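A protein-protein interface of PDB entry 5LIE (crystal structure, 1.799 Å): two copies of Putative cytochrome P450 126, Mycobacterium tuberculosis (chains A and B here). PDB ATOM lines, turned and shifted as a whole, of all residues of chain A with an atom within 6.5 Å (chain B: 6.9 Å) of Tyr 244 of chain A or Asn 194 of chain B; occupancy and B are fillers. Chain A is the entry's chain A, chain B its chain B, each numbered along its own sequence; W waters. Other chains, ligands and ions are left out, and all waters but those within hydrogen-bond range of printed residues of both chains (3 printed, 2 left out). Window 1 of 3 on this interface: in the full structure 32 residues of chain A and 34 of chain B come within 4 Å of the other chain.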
ATOM      1  N   LEU A  88     -17.205 -14.515  -0.961  1.00  0.00           N
ATOM      2  CA  LEU A  88     -15.814 -14.082  -1.102  1.00  0.00           C
ATOM      3  C   LEU A  88     -14.991 -14.705   0.008  1.00  0.00           C
ATOM      4  O   LEU A  88     -15.409 -14.711   1.161  1.00  0.00           O
ATOM      5  CB  LEU A  88     -15.730 -12.536  -0.996  1.00  0.00           C
ATOM      6  CG  LEU A  88     -16.290 -11.727  -2.173  1.00  0.00           C
ATOM      7  CD1 LEU A  88     -16.278 -10.235  -1.817  1.00  0.00           C
ATOM      8  CD2 LEU A  88     -15.476 -11.980  -3.462  1.00  0.00           C
ATOM      9  N   VAL A  90     -12.542 -13.415   1.407  1.00  0.00           N
ATOM     10  CA  VAL A  90     -12.133 -12.440   2.388  1.00  0.00           C
ATOM     11  C   VAL A  90     -13.239 -12.149   3.433  1.00  0.00           C
ATOM     12  O   VAL A  90     -13.062 -11.307   4.326  1.00  0.00           O
ATOM     13  CB  VAL A  90     -11.640 -11.142   1.732  1.00  0.00           C
ATOM     14  CG1 VAL A  90     -10.353 -11.432   0.924  1.00  0.00           C
ATOM     15  CG2 VAL A  90     -12.713 -10.579   0.826  1.00  0.00           C
ATOM     16  N   GLY A 199      -5.093  -1.896 -10.829  1.00  0.00           N
ATOM     17  CA  GLY A 199      -5.474  -2.526  -9.558  1.00  0.00           C
ATOM     18  C   GLY A 199      -4.294  -3.131  -8.828  1.00  0.00           C
ATOM     19  O   GLY A 199      -4.156  -3.013  -7.592  1.00  0.00           O
ATOM     20  N   LEU A 202      -2.226  -0.288  -7.388  1.00  0.00           N
ATOM     21  CA  LEU A 202      -2.875   0.205  -6.140  1.00  0.00           C
ATOM     22  C   LEU A 202      -2.579  -0.729  -4.960  1.00  0.00           C
ATOM     23  O   LEU A 202      -2.215  -0.321  -3.856  1.00  0.00           O
ATOM     24  CB  LEU A 202      -4.392   0.282  -6.340  1.00  0.00           C
ATOM     25  CG  LEU A 202      -5.083   0.756  -5.050  1.00  0.00           C
ATOM     26  CD1 LEU A 202      -4.420   2.082  -4.604  1.00  0.00           C
ATOM     27  CD2 LEU A 202      -6.568   0.928  -5.296  1.00  0.00           C
ATOM     28  N   TYR A 203      -2.769  -2.017  -5.188  1.00  0.00           N
ATOM     29  CA  TYR A 203      -2.443  -3.030  -4.179  1.00  0.00           C
ATOM     30  C   TYR A 203      -0.993  -2.942  -3.717  1.00  0.00           C
ATOM     31  O   TYR A 203      -0.687  -2.897  -2.518  1.00  0.00           O
ATOM     32  CB  TYR A 203      -2.742  -4.406  -4.774  1.00  0.00           C
ATOM     33  CG  TYR A 203      -2.487  -5.558  -3.848  1.00  0.00           C
ATOM     34  CD1 TYR A 203      -3.309  -5.799  -2.740  1.00  0.00           C
ATOM     35  CD2 TYR A 203      -1.438  -6.437  -4.093  1.00  0.00           C
ATOM     36  CE1 TYR A 203      -3.054  -6.901  -1.891  1.00  0.00           C
ATOM     37  CE2 TYR A 203      -1.194  -7.522  -3.275  1.00  0.00           C
ATOM     38  CZ  TYR A 203      -2.009  -7.756  -2.177  1.00  0.00           C
ATOM     39  OH  TYR A 203      -1.746  -8.852  -1.373  1.00  0.00           O
ATOM     40  N   THR A 204      -0.070  -2.907  -4.671  1.00  0.00           N
ATOM     41  CA  THR A 204       1.335  -2.885  -4.348  1.00  0.00           C
ATOM     42  C   THR A 204       1.724  -1.619  -3.598  1.00  0.00           C
ATOM     43  O   THR A 204       2.455  -1.681  -2.635  1.00  0.00           O
ATOM     44  CB  THR A 204       2.160  -3.026  -5.678  1.00  0.00           C
ATOM     45  OG1 THR A 204       1.756  -4.249  -6.295  1.00  0.00           O
ATOM     46  CG2 THR A 204       3.642  -3.072  -5.379  1.00  0.00           C
ATOM     47  N   ALA A 206      -0.342   0.246  -1.786  1.00  0.00           N
ATOM     48  CA  ALA A 206      -0.977   0.188  -0.448  1.00  0.00           C
ATOM     49  C   ALA A 206      -0.121  -0.617   0.494  1.00  0.00           C
ATOM     50  O   ALA A 206       0.090  -0.249   1.638  1.00  0.00           O
ATOM     51  CB  ALA A 206      -2.427  -0.437  -0.534  1.00  0.00           C
ATOM     52  N   LEU A 207       0.396  -1.753   0.039  1.00  0.00           N
ATOM     53  CA  LEU A 207       1.257  -2.560   0.901  1.00  0.00           C
ATOM     54  C   LEU A 207       2.546  -1.801   1.289  1.00  0.00           C
ATOM     55  O   LEU A 207       3.048  -1.957   2.393  1.00  0.00           O
ATOM     56  CB  LEU A 207       1.617  -3.877   0.202  1.00  0.00           C
ATOM     57  CG  LEU A 207       0.454  -4.857  -0.060  1.00  0.00           C
ATOM     58  CD1 LEU A 207       0.990  -6.174  -0.690  1.00  0.00           C
ATOM     59  CD2 LEU A 207      -0.292  -5.166   1.206  1.00  0.00           C
ATOM     60  N   ILE A 210       1.506   0.734   3.967  1.00  0.00           N
ATOM     61  CA  ILE A 210       1.247   0.047   5.226  1.00  0.00           C
ATOM     62  C   ILE A 210       2.582  -0.290   5.915  1.00  0.00           C
ATOM     63  O   ILE A 210       2.766  -0.054   7.097  1.00  0.00           O
ATOM     64  CB  ILE A 210       0.400  -1.242   4.948  1.00  0.00           C
ATOM     65  CG1 ILE A 210      -1.056  -0.866   4.673  1.00  0.00           C
ATOM     66  CG2 ILE A 210       0.495  -2.191   6.047  1.00  0.00           C
ATOM     67  CD1 ILE A 210      -1.861  -1.998   3.918  1.00  0.00           C
ATOM     68  N   LEU A 222      -4.663   4.743   9.179  1.00  0.00           N
ATOM     69  CA  LEU A 222      -3.955   3.534   8.761  1.00  0.00           C
ATOM     70  C   LEU A 222      -2.900   3.174   9.798  1.00  0.00           C
ATOM     71  O   LEU A 222      -2.686   1.999  10.125  1.00  0.00           O
ATOM     72  CB  LEU A 222      -3.330   3.761   7.389  1.00  0.00           C
ATOM     73  CG  LEU A 222      -2.891   2.513   6.631  1.00  0.00           C
ATOM     74  CD1 LEU A 222      -4.014   1.438   6.559  1.00  0.00           C
ATOM     75  CD2 LEU A 222      -2.396   2.953   5.215  1.00  0.00           C
ATOM     76  N   SER A 239      -2.888  -8.739   9.667  1.00  0.00           N
ATOM     77  CA  SER A 239      -1.853  -8.934   8.627  1.00  0.00           C
ATOM     78  C   SER A 239      -1.868  -7.810   7.592  1.00  0.00           C
ATOM     79  O   SER A 239      -2.837  -7.038   7.554  1.00  0.00           O
ATOM     80  CB  SER A 239      -2.152 -10.241   7.877  1.00  0.00           C
ATOM     81  OG  SER A 239      -3.445 -10.144   7.250  1.00  0.00           O
ATOM     82  N   ASP A 240      -0.838  -7.708   6.735  1.00  0.00           N
ATOM     83  CA  ASP A 240      -0.844  -6.684   5.690  1.00  0.00           C
ATOM     84  C   ASP A 240      -2.034  -6.894   4.758  1.00  0.00           C
ATOM     85  O   ASP A 240      -2.629  -5.933   4.271  1.00  0.00           O
ATOM     86  CB  ASP A 240       0.451  -6.684   4.868  1.00  0.00           C
ATOM     87  CG  ASP A 240       1.650  -6.134   5.656  1.00  0.00           C
ATOM     88  OD1 ASP A 240       1.476  -5.755   6.830  1.00  0.00           O
ATOM     89  OD2 ASP A 240       2.762  -6.118   5.104  1.00  0.00           O
ATOM     90  N   ALA A 241      -2.388  -8.156   4.530  1.00  0.00           N
ATOM     91  CA  ALA A 241      -3.547  -8.430   3.667  1.00  0.00           C
ATOM     92  C   ALA A 241      -4.819  -7.867   4.272  1.00  0.00           C
ATOM     93  O   ALA A 241      -5.661  -7.312   3.558  1.00  0.00           O
ATOM     94  CB  ALA A 241      -3.709  -9.938   3.434  1.00  0.00           C
ATOM     95  N   GLU A 242      -4.997  -8.049   5.579  1.00  0.00           N
ATOM     96  CA  GLU A 242      -6.153  -7.462   6.247  1.00  0.00           C
ATOM     97  C   GLU A 242      -6.077  -5.902   6.225  1.00  0.00           C
ATOM     98  O   GLU A 242      -7.080  -5.233   6.052  1.00  0.00           O
ATOM     99  CB  GLU A 242      -6.217  -7.935   7.692  1.00  0.00           C
ATOM    100  CG  GLU A 242      -6.767  -9.368   7.793  1.00  0.00           C
ATOM    101  CD  GLU A 242      -6.372 -10.051   9.108  1.00  0.00           C
ATOM    102  OE1 GLU A 242      -5.167 -10.225   9.355  1.00  0.00           O
ATOM    103  OE2 GLU A 242      -7.247 -10.394   9.903  1.00  0.00           O
ATOM    104  N   LEU A 243      -4.903  -5.337   6.458  1.00  0.00           N
ATOM    105  CA  LEU A 243      -4.748  -3.879   6.355  1.00  0.00           C
ATOM    106  C   LEU A 243      -5.063  -3.367   4.943  1.00  0.00           C
ATOM    107  O   LEU A 243      -5.578  -2.257   4.775  1.00  0.00           O
ATOM    108  CB  LEU A 243      -3.328  -3.464   6.797  1.00  0.00           C
ATOM    109  CG  LEU A 243      -3.114  -3.810   8.292  1.00  0.00           C
ATOM    110  CD1 LEU A 243      -1.637  -3.831   8.688  1.00  0.00           C
ATOM    111  CD2 LEU A 243      -3.887  -2.853   9.192  1.00  0.00           C
ATOM    112  N   TYR A 244      -4.768  -4.155   3.906  1.00  0.00           N
ATOM    113  CA  TYR A 244      -5.130  -3.753   2.550  1.00  0.00           C
ATOM    114  C   TYR A 244      -6.647  -3.723   2.398  1.00  0.00           C
ATOM    115  O   TYR A 244      -7.207  -2.793   1.784  1.00  0.00           O
ATOM    116  CB  TYR A 244      -4.533  -4.683   1.472  1.00  0.00           C
ATOM    117  CG  TYR A 244      -5.083  -4.304   0.159  1.00  0.00           C
ATOM    118  CD1 TYR A 244      -4.683  -3.107  -0.452  1.00  0.00           C
ATOM    119  CD2 TYR A 244      -6.078  -5.068  -0.453  1.00  0.00           C
ATOM    120  CE1 TYR A 244      -5.227  -2.689  -1.637  1.00  0.00           C
ATOM    121  CE2 TYR A 244      -6.613  -4.655  -1.651  1.00  0.00           C
ATOM    122  CZ  TYR A 244      -6.178  -3.461  -2.227  1.00  0.00           C
ATOM    123  OH  TYR A 244      -6.720  -3.029  -3.418  1.00  0.00           O
ATOM    124  N   LEU A 245      -7.321  -4.753   2.906  1.00  0.00           N
ATOM    125  CA  LEU A 245      -8.778  -4.740   2.823  1.00  0.00           C
ATOM    126  C   LEU A 245      -9.367  -3.502   3.480  1.00  0.00           C
ATOM    127  O   LEU A 245     -10.324  -2.939   2.970  1.00  0.00           O
ATOM    128  CB  LEU A 245      -9.376  -5.997   3.462  1.00  0.00           C
ATOM    129  CG  LEU A 245      -8.970  -7.260   2.688  1.00  0.00           C
ATOM    130  CD1 LEU A 245      -9.400  -8.543   3.510  1.00  0.00           C
ATOM    131  CD2 LEU A 245      -9.642  -7.229   1.308  1.00  0.00           C
ATOM    132  N   PHE A 246      -8.809  -3.111   4.623  1.00  0.00           N
ATOM    133  CA  PHE A 246      -9.269  -1.893   5.320  1.00  0.00           C
ATOM    134  C   PHE A 246      -8.969  -0.620   4.477  1.00  0.00           C
ATOM    135  O   PHE A 246      -9.826   0.249   4.300  1.00  0.00           O
ATOM    136  CB  PHE A 246      -8.576  -1.820   6.686  1.00  0.00           C
ATOM    137  CG  PHE A 246      -8.820  -0.515   7.409  1.00  0.00           C
ATOM    138  CD1 PHE A 246     -10.072  -0.209   7.863  1.00  0.00           C
ATOM    139  CD2 PHE A 246      -7.792   0.407   7.555  1.00  0.00           C
ATOM    140  CE1 PHE A 246     -10.307   0.992   8.496  1.00  0.00           C
ATOM    141  CE2 PHE A 246      -8.014   1.606   8.184  1.00  0.00           C
ATOM    142  CZ  PHE A 246      -9.266   1.899   8.657  1.00  0.00           C
ATOM    143  N   PHE A 247      -7.747  -0.515   3.966  1.00  0.00           N
ATOM    144  CA  PHE A 247      -7.365   0.569   3.097  1.00  0.00           C
ATOM    145  C   PHE A 247      -8.370   0.695   1.958  1.00  0.00           C
ATOM    146  O   PHE A 247      -8.853   1.793   1.644  1.00  0.00           O
ATOM    147  CB  PHE A 247      -5.962   0.279   2.525  1.00  0.00           C
ATOM    148  CG  PHE A 247      -5.543   1.224   1.406  1.00  0.00           C
ATOM    149  CD1 PHE A 247      -4.710   2.276   1.681  1.00  0.00           C
ATOM    150  CD2 PHE A 247      -5.926   0.995   0.098  1.00  0.00           C
ATOM    151  CE1 PHE A 247      -4.304   3.147   0.665  1.00  0.00           C
ATOM    152  CE2 PHE A 247      -5.540   1.822  -0.911  1.00  0.00           C
ATOM    153  CZ  PHE A 247      -4.739   2.918  -0.632  1.00  0.00           C
ATOM    154  N   HIS A 248      -8.718  -0.431   1.340  1.00  0.00           N
ATOM    155  CA  HIS A 248      -9.548  -0.339   0.161  1.00  0.00           C
ATOM    156  C   HIS A 248     -10.983   0.015   0.535  1.00  0.00           C
ATOM    157  O   HIS A 248     -11.680   0.694  -0.212  1.00  0.00           O
ATOM    158  CB  HIS A 248      -9.554  -1.640  -0.612  1.00  0.00           C
ATOM    159  CG  HIS A 248     -10.079  -1.469  -2.003  1.00  0.00           C
ATOM    160  ND1 HIS A 248     -11.421  -1.546  -2.311  1.00  0.00           N
ATOM    161  CD2 HIS A 248      -9.440  -1.160  -3.155  1.00  0.00           C
ATOM    162  CE1 HIS A 248     -11.584  -1.303  -3.601  1.00  0.00           C
ATOM    163  NE2 HIS A 248     -10.397  -1.064  -4.134  1.00  0.00           N
ATOM    164  N   LEU A 249     -11.456  -0.497   1.673  1.00  0.00           N
ATOM    165  CA  LEU A 249     -12.791  -0.123   2.168  1.00  0.00           C
ATOM    166  C   LEU A 249     -12.868   1.394   2.259  1.00  0.00           C
ATOM    167  O   LEU A 249     -13.851   2.002   1.827  1.00  0.00           O
ATOM    168  CB  LEU A 249     -13.043  -0.738   3.561  1.00  0.00           C
ATOM    169  CG  LEU A 249     -14.396  -0.393   4.238  1.00  0.00           C
ATOM    170  CD1 LEU A 249     -15.608  -0.864   3.345  1.00  0.00           C
ATOM    171  CD2 LEU A 249     -14.437  -1.044   5.617  1.00  0.00           C
ATOM    172  N   GLN B  86       4.171 -13.222   2.647  1.00  0.00           N
ATOM    173  CA  GLN B  86       2.975 -12.529   3.100  1.00  0.00           C
ATOM    174  C   GLN B  86       1.786 -13.468   3.372  1.00  0.00           C
ATOM    175  O   GLN B  86       1.481 -14.336   2.539  1.00  0.00           O
ATOM    176  CB  GLN B  86       2.557 -11.539   2.040  1.00  0.00           C
ATOM    177  CG  GLN B  86       1.428 -10.721   2.505  1.00  0.00           C
ATOM    178  CD  GLN B  86       1.071  -9.652   1.528  1.00  0.00           C
ATOM    179  OE1 GLN B  86       1.792  -9.418   0.560  1.00  0.00           O
ATOM    180  NE2 GLN B  86      -0.049  -8.982   1.776  1.00  0.00           N
ATOM    181  N   PRO B  89      -5.259 -14.341   2.306  1.00  0.00           N
ATOM    182  CA  PRO B  89      -6.540 -14.941   2.667  1.00  0.00           C
ATOM    183  C   PRO B  89      -7.000 -16.030   1.702  1.00  0.00           C
ATOM    184  O   PRO B  89      -7.982 -16.738   1.985  1.00  0.00           O
ATOM    185  CB  PRO B  89      -7.523 -13.766   2.584  1.00  0.00           C
ATOM    186  CG  PRO B  89      -6.720 -12.569   2.661  1.00  0.00           C
ATOM    187  CD  PRO B  89      -5.352 -12.880   2.112  1.00  0.00           C
ATOM    188  N   VAL B  90      -6.349 -16.134   0.564  1.00  0.00           N
ATOM    189  CA  VAL B  90      -6.691 -17.234  -0.349  1.00  0.00           C
ATOM    190  C   VAL B  90      -6.048 -18.563   0.093  1.00  0.00           C
ATOM    191  O   VAL B  90      -6.248 -19.599  -0.564  1.00  0.00           O
ATOM    192  CB  VAL B  90      -6.285 -16.931  -1.761  1.00  0.00           C
ATOM    193  CG1 VAL B  90      -7.031 -15.662  -2.265  1.00  0.00           C
ATOM    194  CG2 VAL B  90      -4.781 -16.793  -1.896  1.00  0.00           C
ATOM    195  N   ARG B 192      -5.431 -12.823  -6.564  1.00  0.00           N
ATOM    196  CA  ARG B 192      -6.098 -12.198  -5.427  1.00  0.00           C
ATOM    197  C   ARG B 192      -7.556 -12.285  -5.703  1.00  0.00           C
ATOM    198  O   ARG B 192      -7.962 -12.321  -6.848  1.00  0.00           O
ATOM    199  CB  ARG B 192      -5.725 -10.717  -5.338  1.00  0.00           C
ATOM    200  CG  ARG B 192      -4.340 -10.500  -4.857  1.00  0.00           C
ATOM    201  CD  ARG B 192      -4.018  -9.043  -4.908  1.00  0.00           C
ATOM    202  NE  ARG B 192      -3.764  -8.637  -6.270  1.00  0.00           N
ATOM    203  CZ  ARG B 192      -4.361  -7.625  -6.851  1.00  0.00           C
ATOM    204  NH1 ARG B 192      -5.221  -6.928  -6.161  1.00  0.00           N
ATOM    205  NH2 ARG B 192      -4.090  -7.290  -8.101  1.00  0.00           N
ATOM    206  N   LEU B 193      -8.362 -12.267  -4.662  1.00  0.00           N
ATOM    207  CA  LEU B 193      -9.794 -12.145  -4.860  1.00  0.00           C
ATOM    208  C   LEU B 193     -10.287 -11.238  -3.717  1.00  0.00           C
ATOM    209  O   LEU B 193     -10.934 -11.694  -2.797  1.00  0.00           O
ATOM    210  CB  LEU B 193     -10.491 -13.501  -4.798  1.00  0.00           C
ATOM    211  CG  LEU B 193     -11.992 -13.469  -5.164  1.00  0.00           C
ATOM    212  CD1 LEU B 193     -12.278 -12.525  -6.331  1.00  0.00           C
ATOM    213  CD2 LEU B 193     -12.465 -14.881  -5.472  1.00  0.00           C
ATOM    214  N   ASN B 194      -9.933  -9.960  -3.786  1.00  0.00           N
ATOM    215  CA  ASN B 194     -10.370  -9.021  -2.769  1.00  0.00           C
ATOM    216  C   ASN B 194     -11.669  -8.383  -3.250  1.00  0.00           C
ATOM    217  O   ASN B 194     -12.218  -8.757  -4.286  1.00  0.00           O
ATOM    218  CB  ASN B 194      -9.279  -7.999  -2.500  1.00  0.00           C
ATOM    219  CG  ASN B 194      -8.046  -8.644  -1.916  1.00  0.00           C
ATOM    220  OD1 ASN B 194      -8.139  -9.450  -0.982  1.00  0.00           O
ATOM    221  ND2 ASN B 194      -6.894  -8.332  -2.472  1.00  0.00           N
ATOM    222  N   VAL B 195     -12.198  -7.438  -2.501  1.00  0.00           N
ATOM    223  CA  VAL B 195     -13.568  -7.005  -2.807  1.00  0.00           C
ATOM    224  C   VAL B 195     -13.661  -6.370  -4.192  1.00  0.00           C
ATOM    225  O   VAL B 195     -14.620  -6.620  -4.935  1.00  0.00           O
ATOM    226  CB  VAL B 195     -14.107  -6.055  -1.702  1.00  0.00           C
ATOM    227  CG1 VAL B 195     -15.512  -5.626  -2.011  1.00  0.00           C
ATOM    228  CG2 VAL B 195     -14.002  -6.764  -0.354  1.00  0.00           C
ATOM    229  N   GLU B 196     -12.663  -5.582  -4.570  1.00  0.00           N
ATOM    230  CA  GLU B 196     -12.724  -4.895  -5.861  1.00  0.00           C
ATOM    231  C   GLU B 196     -12.599  -5.893  -7.030  1.00  0.00           C
ATOM    232  O   GLU B 196     -12.934  -5.581  -8.175  1.00  0.00           O
ATOM    233  CB  GLU B 196     -11.651  -3.794  -5.964  1.00  0.00           C
ATOM    234  CG  GLU B 196     -10.193  -4.304  -6.087  1.00  0.00           C
ATOM    235  CD  GLU B 196      -9.495  -4.546  -4.744  1.00  0.00           C
ATOM    236  OE1 GLU B 196     -10.174  -4.744  -3.692  1.00  0.00           O
ATOM    237  OE2 GLU B 196      -8.235  -4.571  -4.741  1.00  0.00           O
ATOM    238  N   ASP B 197     -12.136  -7.106  -6.756  1.00  0.00           N
ATOM    239  CA  ASP B 197     -11.998  -8.089  -7.825  1.00  0.00           C
ATOM    240  C   ASP B 197     -13.322  -8.823  -8.116  1.00  0.00           C
ATOM    241  O   ASP B 197     -13.480  -9.355  -9.213  1.00  0.00           O
ATOM    242  CB  ASP B 197     -10.865  -9.076  -7.489  1.00  0.00           C
ATOM    243  CG  ASP B 197      -9.556  -8.363  -7.174  1.00  0.00           C
ATOM    244  OD1 ASP B 197      -9.160  -7.458  -7.964  1.00  0.00           O
ATOM    245  OD2 ASP B 197      -8.909  -8.693  -6.145  1.00  0.00           O
ATOM    246  N   ALA B 198     -14.262  -8.833  -7.157  1.00  0.00           N
ATOM    247  CA  ALA B 198     -15.606  -9.418  -7.349  1.00  0.00           C
ATOM    248  C   ALA B 198     -16.324  -8.848  -8.570  1.00  0.00           C
ATOM    249  O   ALA B 198     -16.416  -7.621  -8.743  1.00  0.00           O
ATOM    250  CB  ALA B 198     -16.512  -9.210  -6.095  1.00  0.00           C
HETATM  251  O   HOH W   1      -6.035  -8.932   1.014  1.00  0.00           O
HETATM  252  O   HOH W   2      -4.396  -9.982  -1.121  1.00  0.00           O
HETATM  253  O   HOH W   3      -6.887  -3.457  -6.722  1.00  0.00           O
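OH of Tyr 244 of chain A is in hydrogen-bond range of OE2 of Glu 196 of chain B.
The side-chain carboxylate (OD2) of Asp 197 of chain B sits at hydrogen-bond distance from the backbone NH (N) of Asn 194 of chain B, 2.9 Å away.
Among the printed residues, pairs that only touch across the chains: His 248 of chain A with Glu 196 of chain B (3.4 Å), Leu 245 of chain A with Asn 194 of chain B (3.5 Å), Val 90 of chain A with Asn 194 of chain B (3.5 Å), Leu 207 of chain A with Gln 86 of chain B (3.6 Å), Tyr 203 of chain A with Gln 86 of chain B (3.6 Å), Tyr 203 of chain A with Arg 192 of chain B (3.6 Å), Ala 241 of chain A with Pro 89 of chain B (3.6 Å), Ala 241 of chain A with Gln 86 of chain B (3.7 Å), Val 90 of chain A with Leu 193 of chain B (3.8 Å), Tyr 244 of chain A with Asn 194 of chain B (3.8 Å), Asp 240 of chain A with Gln 86 of chain B (3.9 Å) and Leu 88 of chain A with Ala 198 of chain B (3.96 Å).
Of the printed residues of chain B, Asp 240 of chain A touches Gln 86 (3.9 Å). Tyr 244 of chain A touches just these residues of chain B: Asn 194 and Glu 196. Of the printed residues of chain A, Ala 198 of chain B touches Leu 88 (3.96 Å). The nearest residue of chain B that does not touch Tyr 244 of chain A is Arg 192 of chain B (5.0 Å).
Among the printed residues, 13 pairs touch across the chains. Among the printed residues, no Asp or Glu carboxylate lies within 4 Å of a Lys or Arg side-chain nitrogen of the other chain.
Position printed for both chains: 90.
Water W3 lies within hydrogen-bond range of the side-chain carboxylate (OE2) of Glu 196 of chain B (2.6 Å), the backbone carbonyl oxygen (O) of Gly 199 of chain A (2.9 Å) and the side-chain hydroxyl (OH) of Tyr 244 of chain A (3.3 Å). Water W2 lies within hydrogen-bond range of the side-chain hydroxyl of Tyr 203 of chain A (2.9 Å) and the side-chain amide nitrogen of Asn 194 of chain B (3.3 Å). Water W1 lies within hydrogen-bond range of the side-chain amide oxygen (OD1) of Asn 194 of chain B and the backbone carbonyl oxygen (O) of Ala 241 of chain A.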
